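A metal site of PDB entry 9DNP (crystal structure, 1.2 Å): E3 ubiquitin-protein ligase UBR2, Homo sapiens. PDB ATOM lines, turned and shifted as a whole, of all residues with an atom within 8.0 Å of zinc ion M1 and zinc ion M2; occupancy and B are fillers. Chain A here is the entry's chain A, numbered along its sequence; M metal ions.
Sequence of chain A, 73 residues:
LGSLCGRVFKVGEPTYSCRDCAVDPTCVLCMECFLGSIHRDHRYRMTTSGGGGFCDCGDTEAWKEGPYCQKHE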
ATOM      1  N   SER A   3      -4.136  12.133  12.959  1.00  0.00           N
ATOM      2  CA  SER A   3      -3.459  11.592  11.784  1.00  0.00           C
ATOM      3  C   SER A   3      -4.497  11.020  10.827  1.00  0.00           C
ATOM      4  O   SER A   3      -5.670  10.843  11.166  1.00  0.00           O
ATOM      5  CB  SER A   3      -2.386  10.550  12.159  1.00  0.00           C
ATOM      6  OG  SER A   3      -2.920   9.532  12.975  1.00  0.00           O
ATOM      7  N   LEU A   4      -4.050  10.759   9.602  1.00  0.00           N
ATOM      8  CA  LEU A   4      -4.958  10.453   8.496  1.00  0.00           C
ATOM      9  C   LEU A   4      -5.113   8.954   8.351  1.00  0.00           C
ATOM     10  O   LEU A   4      -4.125   8.230   8.175  1.00  0.00           O
ATOM     11  CB  LEU A   4      -4.405  11.045   7.201  1.00  0.00           C
ATOM     12  CG  LEU A   4      -5.246  10.997   5.916  1.00  0.00           C
ATOM     13  CD1 LEU A   4      -6.621  11.597   6.119  1.00  0.00           C
ATOM     14  CD2 LEU A   4      -4.529  11.696   4.769  1.00  0.00           C
ATOM     15  N   CYS A   5      -6.365   8.464   8.387  1.00  0.00           N
ATOM     16  CA  CYS A   5      -6.632   7.177   7.759  1.00  0.00           C
ATOM     17  C   CYS A   5      -6.785   7.391   6.259  1.00  0.00           C
ATOM     18  O   CYS A   5      -5.894   7.041   5.487  1.00  0.00           O
ATOM     19  CB  CYS A   5      -7.885   6.484   8.300  1.00  0.00           C
ATOM     20  SG  CYS A   5      -8.184   4.861   7.495  1.00  0.00           S
ATOM     21  N   GLY A   6      -7.952   7.914   5.842  1.00  0.00           N
ATOM     22  CA  GLY A   6      -8.234   8.288   4.476  1.00  0.00           C
ATOM     23  C   GLY A   6      -8.301   7.175   3.459  1.00  0.00           C
ATOM     24  O   GLY A   6      -8.418   7.449   2.267  1.00  0.00           O
ATOM     25  N   ARG A   7      -8.246   5.911   3.885  1.00  0.00           N
ATOM     26  CA  ARG A   7      -7.970   4.847   2.930  1.00  0.00           C
ATOM     27  C   ARG A   7      -9.178   4.510   2.064  1.00  0.00           C
ATOM     28  O   ARG A   7     -10.335   4.624   2.488  1.00  0.00           O
ATOM     29  CB  ARG A   7      -7.447   3.623   3.672  1.00  0.00           C
ATOM     30  CG  ARG A   7      -8.499   2.803   4.350  1.00  0.00           C
ATOM     31  CD  ARG A   7      -7.834   1.504   4.775  1.00  0.00           C
ATOM     32  NE  ARG A   7      -8.730   0.559   5.422  1.00  0.00           N
ATOM     33  CZ  ARG A   7      -9.556  -0.245   4.747  1.00  0.00           C
ATOM     34  NH1 ARG A   7      -9.688  -0.142   3.426  1.00  0.00           N
ATOM     35  NH2 ARG A   7     -10.236  -1.170   5.400  1.00  0.00           N
ATOM     36  N   VAL A   8      -8.894   4.108   0.823  1.00  0.00           N
ATOM     37  CA  VAL A   8      -9.922   3.700  -0.123  1.00  0.00           C
ATOM     38  C   VAL A   8     -10.368   2.289   0.211  1.00  0.00           C
ATOM     39  O   VAL A   8      -9.612   1.492   0.782  1.00  0.00           O
ATOM     40  CB  VAL A   8      -9.343   3.809  -1.560  1.00  0.00           C
ATOM     41  CG1 VAL A   8     -10.285   3.250  -2.624  1.00  0.00           C
ATOM     42  CG2 VAL A   8      -8.950   5.241  -1.864  1.00  0.00           C
ATOM     43  N   PHE A   9     -11.633   1.984  -0.065  1.00  0.00           N
ATOM     44  CA  PHE A   9     -12.154   0.637   0.122  1.00  0.00           C
ATOM     45  C   PHE A   9     -11.958  -0.199  -1.130  1.00  0.00           C
ATOM     46  O   PHE A   9     -12.149   0.283  -2.253  1.00  0.00           O
ATOM     47  CB  PHE A   9     -13.637   0.689   0.482  1.00  0.00           C
ATOM     48  CG  PHE A   9     -13.898   1.227   1.860  1.00  0.00           C
ATOM     49  CD1 PHE A   9     -13.541   0.472   2.964  1.00  0.00           C
ATOM     50  CD2 PHE A   9     -14.445   2.483   2.045  1.00  0.00           C
ATOM     51  CE1 PHE A   9     -13.747   0.953   4.250  1.00  0.00           C
ATOM     52  CE2 PHE A   9     -14.650   2.984   3.341  1.00  0.00           C
ATOM     53  CZ  PHE A   9     -14.285   2.211   4.438  1.00  0.00           C
ATOM     54  N   VAL A  28     -18.802   6.686   6.754  1.00  0.00           N
ATOM     55  CA  VAL A  28     -18.385   5.321   7.064  1.00  0.00           C
ATOM     56  C   VAL A  28     -16.979   5.307   7.644  1.00  0.00           C
ATOM     57  O   VAL A  28     -16.145   6.180   7.378  1.00  0.00           O
ATOM     58  CB  VAL A  28     -18.434   4.370   5.844  1.00  0.00           C
ATOM     59  CG1 VAL A  28     -19.868   4.093   5.460  1.00  0.00           C
ATOM     60  CG2 VAL A  28     -17.666   4.957   4.691  1.00  0.00           C
ATOM     61  N   LEU A  29     -16.716   4.273   8.456  1.00  0.00           N
ATOM     62  CA  LEU A  29     -15.387   3.949   8.951  1.00  0.00           C
ATOM     63  C   LEU A  29     -14.976   2.595   8.402  1.00  0.00           C
ATOM     64  O   LEU A  29     -15.812   1.693   8.223  1.00  0.00           O
ATOM     65  CB  LEU A  29     -15.407   3.853  10.475  1.00  0.00           C
ATOM     66  CG  LEU A  29     -15.750   5.166  11.168  1.00  0.00           C
ATOM     67  CD1 LEU A  29     -15.890   4.916  12.669  1.00  0.00           C
ATOM     68  CD2 LEU A  29     -14.714   6.233  10.885  1.00  0.00           C
ATOM     69  N   CYS A  30     -13.676   2.451   8.124  1.00  0.00           N
ATOM     70  CA  CYS A  30     -13.126   1.154   7.797  1.00  0.00           C
ATOM     71  C   CYS A  30     -13.165   0.264   9.044  1.00  0.00           C
ATOM     72  O   CYS A  30     -13.450   0.724  10.153  1.00  0.00           O
ATOM     73  CB  CYS A  30     -11.693   1.271   7.255  1.00  0.00           C
ATOM     74  SG  CYS A  30     -10.413   1.748   8.443  1.00  0.00           S
ATOM     75  N   MET A  31     -12.877  -1.018   8.851  1.00  0.00           N
ATOM     76  CA  MET A  31     -13.001  -1.955   9.953  1.00  0.00           C
ATOM     77  C   MET A  31     -12.059  -1.601  11.101  1.00  0.00           C
ATOM     78  O   MET A  31     -12.458  -1.574  12.262  1.00  0.00           O
ATOM     79  CB  MET A  31     -12.726  -3.369   9.456  1.00  0.00           C
ATOM     80  CG  MET A  31     -12.781  -4.416  10.535  1.00  0.00           C
ATOM     81  SD  MET A  31     -12.648  -6.068   9.800  1.00  0.00           S
ATOM     82  CE  MET A  31     -12.614  -7.086  11.277  1.00  0.00           C
ATOM     83  N   GLU A  32     -10.809  -1.265  10.776  1.00  0.00           N
ATOM     84  CA  GLU A  32      -9.837  -0.956  11.831  1.00  0.00           C
ATOM     85  C   GLU A  32     -10.274   0.273  12.631  1.00  0.00           C
ATOM     86  O   GLU A  32     -10.183   0.297  13.866  1.00  0.00           O
ATOM     87  CB  GLU A  32      -8.448  -0.754  11.217  1.00  0.00           C
ATOM     88  CG  GLU A  32      -7.439  -0.159  12.168  1.00  0.00           C
ATOM     89  CD  GLU A  32      -6.130   0.244  11.504  1.00  0.00           C
ATOM     90  OE1 GLU A  32      -6.060   0.427  10.259  1.00  0.00           O
ATOM     91  OE2 GLU A  32      -5.170   0.428  12.270  1.00  0.00           O
ATOM     92  N   CYS A  33     -10.741   1.311  11.929  1.00  0.00           N
ATOM     93  CA  CYS A  33     -11.140   2.528  12.619  1.00  0.00           C
ATOM     94  C   CYS A  33     -12.416   2.301  13.420  1.00  0.00           C
ATOM     95  O   CYS A  33     -12.547   2.779  14.553  1.00  0.00           O
ATOM     96  CB  CYS A  33     -11.307   3.656  11.603  1.00  0.00           C
ATOM     97  SG  CYS A  33      -9.701   4.169  10.894  1.00  0.00           S
ATOM     98  N   PHE A  34     -13.359   1.557  12.846  1.00  0.00           N
ATOM     99  CA  PHE A  34     -14.595   1.291  13.581  1.00  0.00           C
ATOM    100  C   PHE A  34     -14.313   0.559  14.881  1.00  0.00           C
ATOM    101  O   PHE A  34     -14.804   0.950  15.941  1.00  0.00           O
ATOM    102  CB  PHE A  34     -15.555   0.481  12.712  1.00  0.00           C
ATOM    103  CG  PHE A  34     -16.829   0.127  13.419  1.00  0.00           C
ATOM    104  CD1 PHE A  34     -17.767   1.113  13.674  1.00  0.00           C
ATOM    105  CD2 PHE A  34     -17.072  -1.167  13.825  1.00  0.00           C
ATOM    106  CE1 PHE A  34     -18.942   0.802  14.324  1.00  0.00           C
ATOM    107  CE2 PHE A  34     -18.256  -1.481  14.471  1.00  0.00           C
ATOM    108  CZ  PHE A  34     -19.183  -0.487  14.721  1.00  0.00           C
ATOM    109  N   GLY A  36     -11.738   0.417  16.665  1.00  0.00           N
ATOM    110  CA  GLY A  36     -10.970   1.202  17.611  1.00  0.00           C
ATOM    111  C   GLY A  36     -11.613   2.520  17.982  1.00  0.00           C
ATOM    112  O   GLY A  36     -10.952   3.410  18.520  1.00  0.00           O
ATOM    113  N   SER A  37     -12.907   2.659  17.693  1.00  0.00           N
ATOM    114  CA  SER A  37     -13.657   3.882  17.959  1.00  0.00           C
ATOM    115  C   SER A  37     -14.725   3.643  19.009  1.00  0.00           C
ATOM    116  O   SER A  37     -15.052   2.506  19.355  1.00  0.00           O
ATOM    117  CB  SER A  37     -14.318   4.404  16.682  1.00  0.00           C
ATOM    118  OG  SER A  37     -15.460   3.634  16.341  1.00  0.00           O
ATOM    119  N   PHE A  54     -14.068   5.963   0.630  1.00  0.00           N
ATOM    120  CA  PHE A  54     -12.943   6.094   1.537  1.00  0.00           C
ATOM    121  C   PHE A  54     -13.444   6.198   2.969  1.00  0.00           C
ATOM    122  O   PHE A  54     -14.579   6.612   3.234  1.00  0.00           O
ATOM    123  CB  PHE A  54     -12.049   7.292   1.191  1.00  0.00           C
ATOM    124  CG  PHE A  54     -12.797   8.607   1.070  1.00  0.00           C
ATOM    125  CD1 PHE A  54     -13.389   8.994  -0.129  1.00  0.00           C
ATOM    126  CD2 PHE A  54     -12.947   9.425   2.167  1.00  0.00           C
ATOM    127  CE1 PHE A  54     -14.075  10.223  -0.219  1.00  0.00           C
ATOM    128  CE2 PHE A  54     -13.639  10.642   2.070  1.00  0.00           C
ATOM    129  CZ  PHE A  54     -14.196  11.021   0.876  1.00  0.00           C
ATOM    130  N   CYS A  55     -12.573   5.840   3.900  1.00  0.00           N
ATOM    131  CA  CYS A  55     -12.868   5.953   5.319  1.00  0.00           C
ATOM    132  C   CYS A  55     -12.928   7.410   5.753  1.00  0.00           C
ATOM    133  O   CYS A  55     -12.076   8.227   5.375  1.00  0.00           O
ATOM    134  CB  CYS A  55     -11.767   5.261   6.093  1.00  0.00           C
ATOM    135  SG  CYS A  55     -11.953   5.270   7.886  1.00  0.00           S
ATOM    136  N   ASP A  56     -13.904   7.714   6.606  1.00  0.00           N
ATOM    137  CA  ASP A  56     -14.125   9.072   7.101  1.00  0.00           C
ATOM    138  C   ASP A  56     -13.578   9.324   8.500  1.00  0.00           C
ATOM    139  O   ASP A  56     -13.952  10.313   9.146  1.00  0.00           O
ATOM    140  CB  ASP A  56     -15.618   9.416   7.052  1.00  0.00           C
ATOM    141  CG  ASP A  56     -16.183   9.387   5.652  1.00  0.00           C
ATOM    142  OD1 ASP A  56     -15.627  10.080   4.769  1.00  0.00           O
ATOM    143  OD2 ASP A  56     -17.197   8.693   5.436  1.00  0.00           O
ATOM    144  N   CYS A  57     -12.728   8.437   8.995  1.00  0.00           N
ATOM    145  CA  CYS A  57     -12.136   8.646  10.317  1.00  0.00           C
ATOM    146  C   CYS A  57     -11.405   9.981  10.346  1.00  0.00           C
ATOM    147  O   CYS A  57     -10.620  10.277   9.445  1.00  0.00           O
ATOM    148  CB  CYS A  57     -11.142   7.538  10.608  1.00  0.00           C
ATOM    149  SG  CYS A  57     -10.382   7.699  12.254  1.00  0.00           S
ATOM    150  N   GLY A  58     -11.697  10.787  11.356  1.00  0.00           N
ATOM    151  CA  GLY A  58     -11.026  12.051  11.507  1.00  0.00           C
ATOM    152  C   GLY A  58     -11.615  13.189  10.719  1.00  0.00           C
ATOM    153  O   GLY A  58     -11.064  14.291  10.741  1.00  0.00           O
ATOM    154  N   PRO A  67     -15.198  11.613  16.214  1.00  0.00           N
ATOM    155  CA  PRO A  67     -14.733  11.536  14.821  1.00  0.00           C
ATOM    156  C   PRO A  67     -13.469  10.718  14.624  1.00  0.00           C
ATOM    157  O   PRO A  67     -13.233  10.236  13.514  1.00  0.00           O
ATOM    158  CB  PRO A  67     -14.516  13.001  14.421  1.00  0.00           C
ATOM    159  CG  PRO A  67     -14.259  13.694  15.729  1.00  0.00           C
ATOM    160  CD  PRO A  67     -15.139  12.995  16.722  1.00  0.00           C
ATOM    161  N   TYR A  68     -12.646  10.543  15.663  1.00  0.00           N
ATOM    162  CA  TYR A  68     -11.354   9.867  15.562  1.00  0.00           C
ATOM    163  C   TYR A  68     -11.388   8.557  16.330  1.00  0.00           C
ATOM    164  O   TYR A  68     -11.920   8.490  17.447  1.00  0.00           O
ATOM    165  CB  TYR A  68     -10.263  10.710  16.219  1.00  0.00           C
ATOM    166  CG  TYR A  68     -10.037  12.050  15.593  1.00  0.00           C
ATOM    167  CD1 TYR A  68      -9.222  12.182  14.475  1.00  0.00           C
ATOM    168  CD2 TYR A  68     -10.653  13.196  16.094  1.00  0.00           C
ATOM    169  CE1 TYR A  68      -9.002  13.422  13.890  1.00  0.00           C
ATOM    170  CE2 TYR A  68     -10.453  14.427  15.511  1.00  0.00           C
ATOM    171  CZ  TYR A  68      -9.627  14.531  14.417  1.00  0.00           C
ATOM    172  OH  TYR A  68      -9.427  15.762  13.835  1.00  0.00           O
ATOM    173  N   CYS A  69     -10.803   7.525  15.728  1.00  0.00           N
ATOM    174  CA  CYS A  69     -10.561   6.275  16.433  1.00  0.00           C
ATOM    175  C   CYS A  69      -9.289   6.402  17.285  1.00  0.00           C
ATOM    176  O   CYS A  69      -8.565   7.400  17.243  1.00  0.00           O
ATOM    177  CB  CYS A  69     -10.445   5.123  15.443  1.00  0.00           C
ATOM    178  SG  CYS A  69      -8.852   5.096  14.567  1.00  0.00           S
ATOM    179  N   GLN A  70      -9.003   5.346  18.058  1.00  0.00           N
ATOM    180  CA  GLN A  70      -7.867   5.364  18.972  1.00  0.00           C
ATOM    181  C   GLN A  70      -6.541   5.570  18.231  1.00  0.00           C
ATOM    182  O   GLN A  70      -5.636   6.205  18.766  1.00  0.00           O
ATOM    183  CB  GLN A  70      -7.834   4.069  19.786  1.00  0.00           C
ATOM    184  CG  GLN A  70      -8.002   2.781  18.966  1.00  0.00           C
ATOM    185  CD  GLN A  70      -8.336   1.532  19.813  1.00  0.00           C
ATOM    186  OE1 GLN A  70      -7.807   0.445  19.590  1.00  0.00           O
ATOM    187  NE2 GLN A  70      -9.245   1.701  20.778  1.00  0.00           N
ATOM    188  N   LYS A  71      -6.429   5.057  17.008  1.00  0.00           N
ATOM    189  CA  LYS A  71      -5.158   5.177  16.303  1.00  0.00           C
ATOM    190  C   LYS A  71      -4.933   6.573  15.748  1.00  0.00           C
ATOM    191  O   LYS A  71      -3.793   7.056  15.714  1.00  0.00           O
ATOM    192  CB  LYS A  71      -5.094   4.156  15.169  1.00  0.00           C
ATOM    193  CG  LYS A  71      -3.813   4.187  14.402  1.00  0.00           C
ATOM    194  CD  LYS A  71      -3.860   3.213  13.251  1.00  0.00           C
ATOM    195  CE  LYS A  71      -2.507   3.033  12.618  1.00  0.00           C
ATOM    196  NZ  LYS A  71      -2.552   1.856  11.712  1.00  0.00           N
ATOM    197  N   HIS A  72      -5.996   7.241  15.290  1.00  0.00           N
ATOM    198  CA  HIS A  72      -5.830   8.446  14.506  1.00  0.00           C
ATOM    199  C   HIS A  72      -6.076   9.723  15.296  1.00  0.00           C
ATOM    200  O   HIS A  72      -5.797  10.806  14.777  1.00  0.00           O
ATOM    201  CB  HIS A  72      -6.709   8.368  13.254  1.00  0.00           C
ATOM    202  CG  HIS A  72      -6.269   7.308  12.308  1.00  0.00           C
ATOM    203  ND1 HIS A  72      -7.068   6.229  11.986  1.00  0.00           N
ATOM    204  CD2 HIS A  72      -5.099   7.113  11.667  1.00  0.00           C
ATOM    205  CE1 HIS A  72      -6.411   5.427  11.159  1.00  0.00           C
ATOM    206  NE2 HIS A  72      -5.205   5.941  10.964  1.00  0.00           N
ATOM    207  N   GLU A  73      -6.557   9.605  16.526  1.00  0.00           N
ATOM    208  CA  GLU A  73      -6.756  10.768  17.376  1.00  0.00           C
ATOM    209  C   GLU A  73      -5.413  11.462  17.674  1.00  0.00           C
ATOM    210  O   GLU A  73      -5.391  12.626  18.059  1.00  0.00           O
ATOM    211  CB  GLU A  73      -7.480  10.364  18.661  1.00  0.00           C
ATOM    212  CG  GLU A  73      -6.653   9.521  19.624  1.00  0.00           C
ATOM    213  CD  GLU A  73      -7.444   9.103  20.862  1.00  0.00           C
ATOM    214  OE1 GLU A  73      -6.883   8.381  21.715  1.00  0.00           O
ATOM    215  OE2 GLU A  73      -8.616   9.505  20.977  1.00  0.00           O
ATOM    216  OXT GLU A  73      -4.332  10.882  17.510  1.00  0.00           O
HETATM  217 ZN    ZN M   1      -9.064   5.855  12.403  1.00  0.00          ZN
HETATM  218 ZN    ZN M   2     -10.093   4.056   8.523  1.00  0.00          ZN
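Zinc ion M1 is bound by a ring nitrogen (ND1) of His 72 (2.1 Å), the side-chain sulfur of Cys 57 (2.3 Å), the side-chain sulfur of Cys 69 (2.3 Å) and the side-chain sulfur of Cys 33 (2.4 Å).
Zinc ion M1 has four donor atoms within binding distance.
Zinc ion M2 is bound by the side-chain sulfur (SG) of Cys 55 (2.3 Å), the side-chain sulfur (SG) of Cys 5 (2.3 Å), the side-chain sulfur (SG) of Cys 30 (2.3 Å) and the side-chain sulfur (SG) of Cys 33 (2.4 Å).
Zinc ion M2 has four donor atoms within binding distance.
The backbone NH (N) of Ser 3 sits at hydrogen-bond distance from the backbone carbonyl oxygen (O) of His 72 (2.8 Å).
The backbone NH (N) of Cys 57 sits close to the side-chain sulfur (SG) of Cys 55, 3.4 Å away.
SG of Cys 69 lies close to N of Lys 71, at 3.4 Å.
The backbone carbonyl oxygen (O) of Arg 7 lies within hydrogen-bond range of the backbone NH (N) of Cys 55.
The side-chain sulfur (SG) of Cys 5 lies close to the backbone NH (N) of Arg 7, 3.8 Å away.
The guanidinium group (NE) of Arg 7 sits close to the side-chain sulfur (SG) of Cys 30, at 3.7 Å.
Four residues have an atom within 4 Å of zinc ion M2: Cys 5, Cys 30, Cys 33 and Cys 55.
The nearest printed residue that does not touch zinc ion M2 is Cys 57 (4.2 Å).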
